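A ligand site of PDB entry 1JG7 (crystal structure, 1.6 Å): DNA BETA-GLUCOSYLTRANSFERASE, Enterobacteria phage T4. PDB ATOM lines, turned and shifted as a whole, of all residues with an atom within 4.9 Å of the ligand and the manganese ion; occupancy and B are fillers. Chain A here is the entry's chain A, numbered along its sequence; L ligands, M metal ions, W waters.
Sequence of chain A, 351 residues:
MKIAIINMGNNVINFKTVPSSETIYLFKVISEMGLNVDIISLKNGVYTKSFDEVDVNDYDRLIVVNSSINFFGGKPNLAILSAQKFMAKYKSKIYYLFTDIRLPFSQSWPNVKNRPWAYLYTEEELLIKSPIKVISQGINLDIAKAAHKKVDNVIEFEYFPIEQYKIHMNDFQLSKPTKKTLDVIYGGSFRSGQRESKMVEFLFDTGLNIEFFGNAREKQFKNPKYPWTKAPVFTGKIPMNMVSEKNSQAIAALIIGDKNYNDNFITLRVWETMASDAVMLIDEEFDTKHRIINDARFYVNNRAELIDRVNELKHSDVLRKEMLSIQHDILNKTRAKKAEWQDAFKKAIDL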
ATOM      1  N   VAL A  18      -6.423   9.298   1.887  1.00  0.00           N
ATOM      2  CA  VAL A  18      -5.405   9.821   1.001  1.00  0.00           C
ATOM      3  C   VAL A  18      -4.403   8.768   0.526  1.00  0.00           C
ATOM      4  O   VAL A  18      -4.099   8.677  -0.667  1.00  0.00           O
ATOM      5  CB  VAL A  18      -4.650  11.000   1.636  1.00  0.00           C
ATOM      6  CG1 VAL A  18      -3.504  11.438   0.740  1.00  0.00           C
ATOM      7  CG2 VAL A  18      -5.618  12.176   1.848  1.00  0.00           C
ATOM      8  N   THR A  99       7.445  10.619  -2.185  1.00  0.00           N
ATOM      9  CA  THR A  99       6.669  11.839  -2.412  1.00  0.00           C
ATOM     10  C   THR A  99       6.508  12.719  -1.166  1.00  0.00           C
ATOM     11  O   THR A  99       6.077  13.871  -1.257  1.00  0.00           O
ATOM     12  CB  THR A  99       5.253  11.505  -2.941  1.00  0.00           C
ATOM     13  OG1 THR A  99       4.531  10.769  -1.943  1.00  0.00           O
ATOM     14  CG2 THR A  99       5.326  10.679  -4.215  1.00  0.00           C
ATOM     15  N   ASP A 100       6.845  12.168  -0.007  1.00  0.00           N
ATOM     16  CA  ASP A 100       6.720  12.886   1.265  1.00  0.00           C
ATOM     17  C   ASP A 100       8.033  12.726   2.027  1.00  0.00           C
ATOM     18  O   ASP A 100       8.421  11.600   2.350  1.00  0.00           O
ATOM     19  CB  ASP A 100       5.548  12.302   2.059  1.00  0.00           C
ATOM     20  CG  ASP A 100       5.233  13.071   3.324  1.00  0.00           C
ATOM     21  OD1 ASP A 100       4.055  13.076   3.739  1.00  0.00           O
ATOM     22  OD2 ASP A 100       6.152  13.669   3.930  1.00  0.00           O
ATOM     23  N   GLU A 163       4.058  13.235  -8.747  1.00  0.00           N
ATOM     24  CA  GLU A 163       2.731  13.812  -8.540  1.00  0.00           C
ATOM     25  C   GLU A 163       2.139  14.628  -9.670  1.00  0.00           C
ATOM     26  O   GLU A 163       1.077  15.238  -9.524  1.00  0.00           O
ATOM     27  CB  GLU A 163       2.706  14.556  -7.204  1.00  0.00           C
ATOM     28  CG  GLU A 163       3.036  13.582  -6.050  1.00  0.00           C
ATOM     29  CD  GLU A 163       2.728  14.095  -4.655  1.00  0.00           C
ATOM     30  OE1 GLU A 163       3.003  15.267  -4.347  1.00  0.00           O
ATOM     31  OE2 GLU A 163       2.220  13.291  -3.842  1.00  0.00           O
ATOM     32  N   TYR A 186      -7.332  26.058   1.966  1.00  0.00           N
ATOM     33  CA  TYR A 186      -6.170  25.177   2.013  1.00  0.00           C
ATOM     34  C   TYR A 186      -6.642  23.834   2.571  1.00  0.00           C
ATOM     35  O   TYR A 186      -7.339  23.799   3.578  1.00  0.00           O
ATOM     36  CB  TYR A 186      -5.068  25.753   2.912  1.00  0.00           C
ATOM     37  CG  TYR A 186      -3.912  24.796   3.158  1.00  0.00           C
ATOM     38  CD1 TYR A 186      -3.938  23.881   4.205  1.00  0.00           C
ATOM     39  CD2 TYR A 186      -2.782  24.828   2.337  1.00  0.00           C
ATOM     40  CE1 TYR A 186      -2.872  23.013   4.445  1.00  0.00           C
ATOM     41  CE2 TYR A 186      -1.706  23.964   2.557  1.00  0.00           C
ATOM     42  CZ  TYR A 186      -1.756  23.063   3.620  1.00  0.00           C
ATOM     43  OH  TYR A 186      -0.680  22.215   3.839  1.00  0.00           O
ATOM     44  N   GLY A 187      -6.258  22.747   1.899  1.00  0.00           N
ATOM     45  CA  GLY A 187      -6.640  21.418   2.372  1.00  0.00           C
ATOM     46  C   GLY A 187      -5.451  20.520   2.646  1.00  0.00           C
ATOM     47  O   GLY A 187      -4.538  20.425   1.826  1.00  0.00           O
ATOM     48  N   GLY A 188      -5.471  19.857   3.795  1.00  0.00           N
ATOM     49  CA  GLY A 188      -4.377  18.957   4.149  1.00  0.00           C
ATOM     50  C   GLY A 188      -4.432  18.506   5.606  1.00  0.00           C
ATOM     51  O   GLY A 188      -5.360  18.843   6.346  1.00  0.00           O
ATOM     52  N   SER A 189      -3.428  17.734   6.011  1.00  0.00           N
ATOM     53  CA  SER A 189      -3.366  17.250   7.382  1.00  0.00           C
ATOM     54  C   SER A 189      -2.491  18.193   8.222  1.00  0.00           C
ATOM     55  O   SER A 189      -1.954  19.173   7.716  1.00  0.00           O
ATOM     56  CB  SER A 189      -2.770  15.845   7.429  1.00  0.00           C
ATOM     57  OG  SER A 189      -1.380  15.875   7.144  1.00  0.00           O
ATOM     58  N   ARG A 191       0.197  17.295   9.507  1.00  0.00           N
ATOM     59  CA  ARG A 191       1.558  16.873   9.220  1.00  0.00           C
ATOM     60  C   ARG A 191       2.460  16.897  10.444  1.00  0.00           C
ATOM     61  O   ARG A 191       3.617  17.328  10.376  1.00  0.00           O
ATOM     62  CB  ARG A 191       2.160  17.738   8.117  1.00  0.00           C
ATOM     63  CG  ARG A 191       1.514  17.515   6.752  1.00  0.00           C
ATOM     64  CD  ARG A 191       2.276  18.237   5.669  1.00  0.00           C
ATOM     65  NE  ARG A 191       3.665  17.776   5.550  1.00  0.00           N
ATOM     66  CZ  ARG A 191       4.029  16.591   5.087  1.00  0.00           C
ATOM     67  NH1 ARG A 191       3.119  15.718   4.658  1.00  0.00           N
ATOM     68  NH2 ARG A 191       5.315  16.276   5.017  1.00  0.00           N
ATOM     69  N   ARG A 195       4.618  21.909   9.710  1.00  0.00           N
ATOM     70  CA  ARG A 195       4.313  23.073   8.894  1.00  0.00           C
ATOM     71  C   ARG A 195       3.474  24.099   9.655  1.00  0.00           C
ATOM     72  O   ARG A 195       2.875  24.999   9.053  1.00  0.00           O
ATOM     73  CB  ARG A 195       3.556  22.607   7.639  1.00  0.00           C
ATOM     74  CG  ARG A 195       3.526  23.584   6.481  1.00  0.00           C
ATOM     75  CD  ARG A 195       2.832  22.964   5.273  1.00  0.00           C
ATOM     76  NE  ARG A 195       3.562  21.821   4.744  1.00  0.00           N
ATOM     77  CZ  ARG A 195       3.148  21.064   3.726  1.00  0.00           C
ATOM     78  NH1 ARG A 195       1.994  21.309   3.129  1.00  0.00           N
ATOM     79  NH2 ARG A 195       3.910  20.062   3.296  1.00  0.00           N
ATOM     80  N   PHE A 213      -9.553  22.697   5.105  1.00  0.00           N
ATOM     81  CA  PHE A 213     -10.173  21.380   5.085  1.00  0.00           C
ATOM     82  C   PHE A 213      -9.112  20.295   5.220  1.00  0.00           C
ATOM     83  O   PHE A 213      -7.919  20.588   5.123  1.00  0.00           O
ATOM     84  CB  PHE A 213     -11.070  21.175   3.849  1.00  0.00           C
ATOM     85  CG  PHE A 213     -10.348  21.171   2.518  1.00  0.00           C
ATOM     86  CD1 PHE A 213      -9.991  22.361   1.889  1.00  0.00           C
ATOM     87  CD2 PHE A 213     -10.109  19.973   1.855  1.00  0.00           C
ATOM     88  CE1 PHE A 213      -9.412  22.354   0.619  1.00  0.00           C
ATOM     89  CE2 PHE A 213      -9.530  19.949   0.586  1.00  0.00           C
ATOM     90  CZ  PHE A 213      -9.175  21.146  -0.027  1.00  0.00           C
ATOM     91  N   GLY A 214      -9.529  19.057   5.462  1.00  0.00           N
ATOM     92  CA  GLY A 214      -8.572  17.978   5.632  1.00  0.00           C
ATOM     93  C   GLY A 214      -8.581  17.423   7.046  1.00  0.00           C
ATOM     94  O   GLY A 214      -9.423  17.799   7.855  1.00  0.00           O
ATOM     95  N   GLY A 236     -13.132  19.548   8.021  1.00  0.00           N
ATOM     96  CA  GLY A 236     -13.004  18.104   7.923  1.00  0.00           C
ATOM     97  C   GLY A 236     -12.511  17.608   6.586  1.00  0.00           C
ATOM     98  O   GLY A 236     -12.363  18.370   5.630  1.00  0.00           O
ATOM     99  N   LYS A 237     -12.282  16.308   6.504  1.00  0.00           N
ATOM    100  CA  LYS A 237     -11.763  15.711   5.287  1.00  0.00           C
ATOM    101  C   LYS A 237     -12.794  15.429   4.197  1.00  0.00           C
ATOM    102  O   LYS A 237     -14.002  15.374   4.445  1.00  0.00           O
ATOM    103  CB  LYS A 237     -11.046  14.403   5.629  1.00  0.00           C
ATOM    104  CG  LYS A 237     -11.997  13.289   6.058  1.00  0.00           C
ATOM    105  CD  LYS A 237     -11.257  12.010   6.397  1.00  0.00           C
ATOM    106  CE  LYS A 237     -10.517  11.459   5.190  1.00  0.00           C
ATOM    107  NZ  LYS A 237      -9.838  10.172   5.493  1.00  0.00           N
ATOM    108  N   ILE A 238     -12.281  15.273   2.982  1.00  0.00           N
ATOM    109  CA  ILE A 238     -13.090  14.932   1.817  1.00  0.00           C
ATOM    110  C   ILE A 238     -12.230  14.019   0.962  1.00  0.00           C
ATOM    111  O   ILE A 238     -11.015  13.942   1.152  1.00  0.00           O
ATOM    112  CB  ILE A 238     -13.467  16.182   0.973  1.00  0.00           C
ATOM    113  CG1 ILE A 238     -12.205  16.861   0.434  1.00  0.00           C
ATOM    114  CG2 ILE A 238     -14.309  17.128   1.802  1.00  0.00           C
ATOM    115  CD1 ILE A 238     -12.489  17.975  -0.549  1.00  0.00           C
ATOM    116  N   PRO A 239     -12.844  13.302   0.011  1.00  0.00           N
ATOM    117  CA  PRO A 239     -12.096  12.391  -0.858  1.00  0.00           C
ATOM    118  C   PRO A 239     -11.108  13.140  -1.754  1.00  0.00           C
ATOM    119  O   PRO A 239     -11.389  14.253  -2.199  1.00  0.00           O
ATOM    120  CB  PRO A 239     -13.191  11.689  -1.667  1.00  0.00           C
ATOM    121  CG  PRO A 239     -14.370  11.725  -0.729  1.00  0.00           C
ATOM    122  CD  PRO A 239     -14.296  13.141  -0.199  1.00  0.00           C
ATOM    123  N   MET A 240      -9.972  12.516  -2.039  1.00  0.00           N
ATOM    124  CA  MET A 240      -8.971  13.147  -2.887  1.00  0.00           C
ATOM    125  C   MET A 240      -9.527  13.530  -4.256  1.00  0.00           C
ATOM    126  O   MET A 240      -9.093  14.518  -4.842  1.00  0.00           O
ATOM    127  CB  MET A 240      -7.761  12.228  -3.066  1.00  0.00           C
ATOM    128  CG  MET A 240      -6.665  12.819  -3.936  1.00  0.00           C
ATOM    129  SD  MET A 240      -5.267  11.694  -4.165  1.00  0.00           S
ATOM    130  CE  MET A 240      -4.596  12.302  -5.679  1.00  0.00           C
ATOM    131  N   VAL A 243     -11.088  17.147  -4.296  1.00  0.00           N
ATOM    132  CA  VAL A 243     -10.258  18.266  -3.874  1.00  0.00           C
ATOM    133  C   VAL A 243     -10.271  19.494  -4.787  1.00  0.00           C
ATOM    134  O   VAL A 243     -10.375  20.621  -4.300  1.00  0.00           O
ATOM    135  CB  VAL A 243      -8.789  17.818  -3.658  1.00  0.00           C
ATOM    136  CG1 VAL A 243      -7.883  19.016  -3.436  1.00  0.00           C
ATOM    137  CG2 VAL A 243      -8.722  16.897  -2.451  1.00  0.00           C
ATOM    138  N   ILE A 256       1.905  25.945   0.242  1.00  0.00           N
ATOM    139  CA  ILE A 256       3.005  26.011   1.202  1.00  0.00           C
ATOM    140  C   ILE A 256       3.535  24.597   1.316  1.00  0.00           C
ATOM    141  O   ILE A 256       2.919  23.656   0.806  1.00  0.00           O
ATOM    142  CB  ILE A 256       2.545  26.483   2.611  1.00  0.00           C
ATOM    143  CG1 ILE A 256       1.281  25.726   3.033  1.00  0.00           C
ATOM    144  CG2 ILE A 256       2.345  27.996   2.612  1.00  0.00           C
ATOM    145  CD1 ILE A 256       0.849  25.992   4.476  1.00  0.00           C
ATOM    146  N   TYR A 261      10.857  21.027   1.407  1.00  0.00           N
ATOM    147  CA  TYR A 261      10.213  20.942   0.100  1.00  0.00           C
ATOM    148  C   TYR A 261      10.639  22.141  -0.736  1.00  0.00           C
ATOM    149  O   TYR A 261      10.614  22.097  -1.969  1.00  0.00           O
ATOM    150  CB  TYR A 261       8.687  20.967   0.224  1.00  0.00           C
ATOM    151  CG  TYR A 261       8.066  19.637   0.605  1.00  0.00           C
ATOM    152  CD1 TYR A 261       8.811  18.460   0.572  1.00  0.00           C
ATOM    153  CD2 TYR A 261       6.722  19.550   0.967  1.00  0.00           C
ATOM    154  CE1 TYR A 261       8.243  17.234   0.894  1.00  0.00           C
ATOM    155  CE2 TYR A 261       6.140  18.324   1.287  1.00  0.00           C
ATOM    156  CZ  TYR A 261       6.914  17.180   1.254  1.00  0.00           C
ATOM    157  OH  TYR A 261       6.359  15.954   1.577  1.00  0.00           O
ATOM    158  N   THR A 267       4.757  19.664  -5.359  1.00  0.00           N
ATOM    159  CA  THR A 267       3.759  18.743  -4.869  1.00  0.00           C
ATOM    160  C   THR A 267       2.422  18.675  -5.582  1.00  0.00           C
ATOM    161  O   THR A 267       2.058  19.548  -6.367  1.00  0.00           O
ATOM    162  CB  THR A 267       3.474  19.024  -3.397  1.00  0.00           C
ATOM    163  OG1 THR A 267       3.096  20.397  -3.257  1.00  0.00           O
ATOM    164  CG2 THR A 267       4.725  18.757  -2.555  1.00  0.00           C
ATOM    165  N   LEU A 268       1.686  17.610  -5.270  1.00  0.00           N
ATOM    166  CA  LEU A 268       0.370  17.362  -5.841  1.00  0.00           C
ATOM    167  C   LEU A 268      -0.546  18.577  -5.692  1.00  0.00           C
ATOM    168  O   LEU A 268      -1.271  18.909  -6.623  1.00  0.00           O
ATOM    169  CB  LEU A 268      -0.264  16.145  -5.161  1.00  0.00           C
ATOM    170  CG  LEU A 268      -1.698  15.759  -5.548  1.00  0.00           C
ATOM    171  CD1 LEU A 268      -1.769  15.429  -7.027  1.00  0.00           C
ATOM    172  CD2 LEU A 268      -2.138  14.561  -4.714  1.00  0.00           C
ATOM    173  N   ARG A 269      -0.492  19.252  -4.538  1.00  0.00           N
ATOM    174  CA  ARG A 269      -1.360  20.401  -4.328  1.00  0.00           C
ATOM    175  C   ARG A 269      -1.100  21.522  -5.326  1.00  0.00           C
ATOM    176  O   ARG A 269      -1.992  22.307  -5.604  1.00  0.00           O
ATOM    177  CB  ARG A 269      -1.280  20.953  -2.892  1.00  0.00           C
ATOM    178  CG  ARG A 269      -0.039  21.728  -2.558  1.00  0.00           C
ATOM    179  CD  ARG A 269      -0.175  22.425  -1.195  1.00  0.00           C
ATOM    180  NE  ARG A 269      -0.436  21.486  -0.101  1.00  0.00           N
ATOM    181  CZ  ARG A 269      -1.640  21.264   0.434  1.00  0.00           C
ATOM    182  NH1 ARG A 269      -2.700  21.919  -0.001  1.00  0.00           N
ATOM    183  NH2 ARG A 269      -1.766  20.382   1.428  1.00  0.00           N
ATOM    184  N   GLU A 272      -3.304  20.416  -8.161  1.00  0.00           N
ATOM    185  CA  GLU A 272      -4.727  20.431  -7.773  1.00  0.00           C
ATOM    186  C   GLU A 272      -5.235  21.857  -7.666  1.00  0.00           C
ATOM    187  O   GLU A 272      -6.411  22.131  -7.909  1.00  0.00           O
ATOM    188  CB  GLU A 272      -4.944  19.773  -6.425  1.00  0.00           C
ATOM    189  CG  GLU A 272      -4.520  18.332  -6.318  1.00  0.00           C
ATOM    190  CD  GLU A 272      -4.677  17.816  -4.913  1.00  0.00           C
ATOM    191  OE1 GLU A 272      -4.289  18.556  -3.968  1.00  0.00           O
ATOM    192  OE2 GLU A 272      -5.168  16.680  -4.739  1.00  0.00           O
HETATM  193  N1  LIG L   1      -6.396  15.888   0.636  1.00  0.00           N
HETATM  194  C1  LIG L   1      -7.524  15.090   0.480  1.00  0.00           C
HETATM  195  N2  LIG L   1      -8.598  15.451   1.249  1.00  0.00           N
HETATM  196  C2  LIG L   1      -8.674  16.524   2.129  1.00  0.00           C
HETATM  197  C3  LIG L   1      -7.485  17.318   2.199  1.00  0.00           C
HETATM  198  C4  LIG L   1      -6.417  16.978   1.476  1.00  0.00           C
HETATM  199  O1  LIG L   1      -7.554  14.129  -0.279  1.00  0.00           O
HETATM  200  O2  LIG L   1      -9.683  16.691   2.816  1.00  0.00           O
HETATM  201  C5  LIG L   1      -5.183  15.524  -0.115  1.00  0.00           C
HETATM  202  C6  LIG L   1      -4.939  16.368  -1.372  1.00  0.00           C
HETATM  203  O3  LIG L   1      -4.668  15.522  -2.467  1.00  0.00           O
HETATM  204  C7  LIG L   1      -3.755  17.237  -0.967  1.00  0.00           C
HETATM  205  C8  LIG L   1      -3.012  16.354   0.027  1.00  0.00           C
HETATM  206  O4  LIG L   1      -4.069  15.680   0.748  1.00  0.00           O
HETATM  207  O5  LIG L   1      -2.887  17.540  -2.051  1.00  0.00           O
HETATM  208  C9  LIG L   1      -2.162  17.152   0.987  1.00  0.00           C
HETATM  209  O6  LIG L   1      -1.355  16.277   1.761  1.00  0.00           O
HETATM  210  P1  LIG L   1      -0.490  16.862   2.961  1.00  0.00           P
HETATM  211  O7  LIG L   1      -1.408  17.458   3.948  1.00  0.00           O
HETATM  212  O8  LIG L   1       0.479  15.815   3.386  1.00  0.00           O
HETATM  213  O9  LIG L   1       0.281  18.099   2.276  1.00  0.00           O
HETATM  214  P2  LIG L   1       1.520  18.148   1.269  1.00  0.00           P
HETATM  215  O10 LIG L   1       2.653  17.880   2.200  1.00  0.00           O
HETATM  216  O11 LIG L   1       1.408  19.547   0.770  1.00  0.00           O
HETATM  217  O12 LIG L   1       1.209  17.078   0.291  1.00  0.00           O
HETATM  218 MN    MN M   1       2.139  15.245  -0.174  1.00  0.00          MN
HETATM  219  O   HOH W   1      -1.073  19.904   5.110  1.00  0.00           O
HETATM  220  O   HOH W   2      -3.387  13.308  -2.092  1.00  0.00           O
HETATM  221  O   HOH W   3       0.019  17.897  -2.041  1.00  0.00           O
HETATM  222  O   HOH W   4       3.007  13.206  -0.629  1.00  0.00           O
HETATM  223  O   HOH W   5       1.726  15.869  -2.084  1.00  0.00           O
HETATM  224  O   HOH W   6       3.872  15.584   1.290  1.00  0.00           O
HETATM  225  O   HOH W   7       3.143  21.137  -0.558  1.00  0.00           O
HETATM  226  O   HOH W   8       4.168  15.563  -1.359  1.00  0.00           O
HETATM  227  O   HOH W   9       1.709  14.389   1.717  1.00  0.00           O
HETATM  228  O   HOH W  10      -3.907  15.230   3.544  1.00  0.00           O
HETATM  229  O   HOH W  11      -0.291  14.018   0.268  1.00  0.00           O
HETATM  230  O   HOH W  12       0.970  13.292  -1.825  1.00  0.00           O
HETATM  231  O   HOH W  13      -0.354  14.131   5.354  1.00  0.00           O
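The side-chain carboxylate (OE1) of Glu 272 sits at hydrogen-bond distance from an oxygen (O5) of the ligand, 2.6 Å away. O10 of the ligand lies within salt-bridge range of NH2 of Arg 195 (2.7 Å). NE of Arg 269 is in salt-bridge range of O11 of the ligand (2.8 Å). An oxygen (O2) of the ligand lies within hydrogen-bond range of the backbone NH (N) of Ile 238. O of Ile 238 lies within hydrogen-bond range of N2 of the ligand (2.9 Å). The backbone NH (N) of Ser 189 sits at hydrogen-bond distance from an oxygen (O7) of the ligand. An oxygen (O8) of the ligand is in salt-bridge range of the guanidinium group (NH1) of Arg 191 (2.9 Å). An oxygen (O1) of the ligand lies close to the backbone NH of Met 240, 3.4 Å away.
The backbone carbonyl oxygen (O) of Ile 256 is in hydrogen-bond range of the guanidinium group (NH1) of Arg 195, at 3.4 Å. The side-chain hydroxyl (OH) of Tyr 186 lies within hydrogen-bond range of the guanidinium group (NH1) of Arg 195 (2.9 Å). The backbone NH (N) of Arg 191 lies close to the side-chain hydroxyl (OG) of Ser 189 (3.2 Å). NH2 of Arg 191 is in salt-bridge range of OD2 of Asp 100 (2.9 Å). The backbone carbonyl oxygen (O) of Gly 214 is in hydrogen-bond range of the backbone NH (N) of Lys 237. N of Gly 214 is in hydrogen-bond range of O of Gly 236, at 2.9 Å. The backbone NH of Gly 188 is in hydrogen-bond range of the backbone carbonyl oxygen of Phe 213, at 2.9 Å. The backbone NH (N) of Phe 213 sits at hydrogen-bond distance from the backbone carbonyl oxygen (O) of Tyr 186, 2.9 Å away.
Val 18 touches the ligand (CG2 to O1, 3.5 Å). C of Gly 187 touches C3 of the ligand, at 3.8 Å. CA of Gly 188 touches O7 of the ligand, 3.3 Å away. Phe 213 touches the ligand. Gly 214 touches the ligand. CA of Lys 237 touches O2 of the ligand, 3.4 Å away. Pro 239 touches the ligand (C to O1, 3.97 Å). Val 243 touches the ligand. Tyr 261 touches the ligand (CE2 to O10, 3.6 Å). Leu 268 touches the ligand (CD2 to O3, 3.5 Å). Hydrophobic or aromatic side chains within 4 Å of the ligand: Val 18, Phe 213, Ile 238, Met 240, Val 243, Tyr 261 and Leu 268. Within 4 Å of the ligand: Val 18, Gly 187, Gly 188, Ser 189, Arg 191, Arg 195, Phe 213, Gly 214, Lys 237, Ile 238, Pro 239, Met 240, Val 243, Tyr 261, Leu 268, Arg 269 and Glu 272.
Water W8 lies within hydrogen-bond range of O of Thr 99 (2.6 Å) and OE1 of Glu 163 (3.2 Å). Water W2 lies within hydrogen-bond range of O3 of the ligand (2.6 Å) and SD of Met 240 (3.2 Å). Water W7 lies within hydrogen-bond range of an oxygen (O11) of the ligand (2.7 Å), the side-chain hydroxyl of Thr 267 (2.8 Å) and the backbone carbonyl oxygen of Ile 256 (2.9 Å). Water W13 lies within hydrogen-bond range of OG of Ser 189 and O8 of the ligand. Water W1 lies within hydrogen-bond range of OH of Tyr 186, O7 of the ligand and O of Ser 189. Water W3 lies within hydrogen-bond range of the backbone NH (N) of Arg 269 (2.9 Å) and an oxygen (O5) of the ligand (2.9 Å).
No residue comes within 4 Å of the manganese ion.
The manganese ion is bound by water W5 (2.1 Å), an oxygen (O12) of the ligand (2.1 Å), water W9 (2.1 Å), water W4 (2.3 Å), water W6 (2.3 Å) and water W8 (2.4 Å). The manganese ion has six donor atoms within binding distance. Slightly farther from the manganese ion lies water W11 (2.8 Å). Slightly farther from the manganese ion lies water W12 (2.8 Å).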
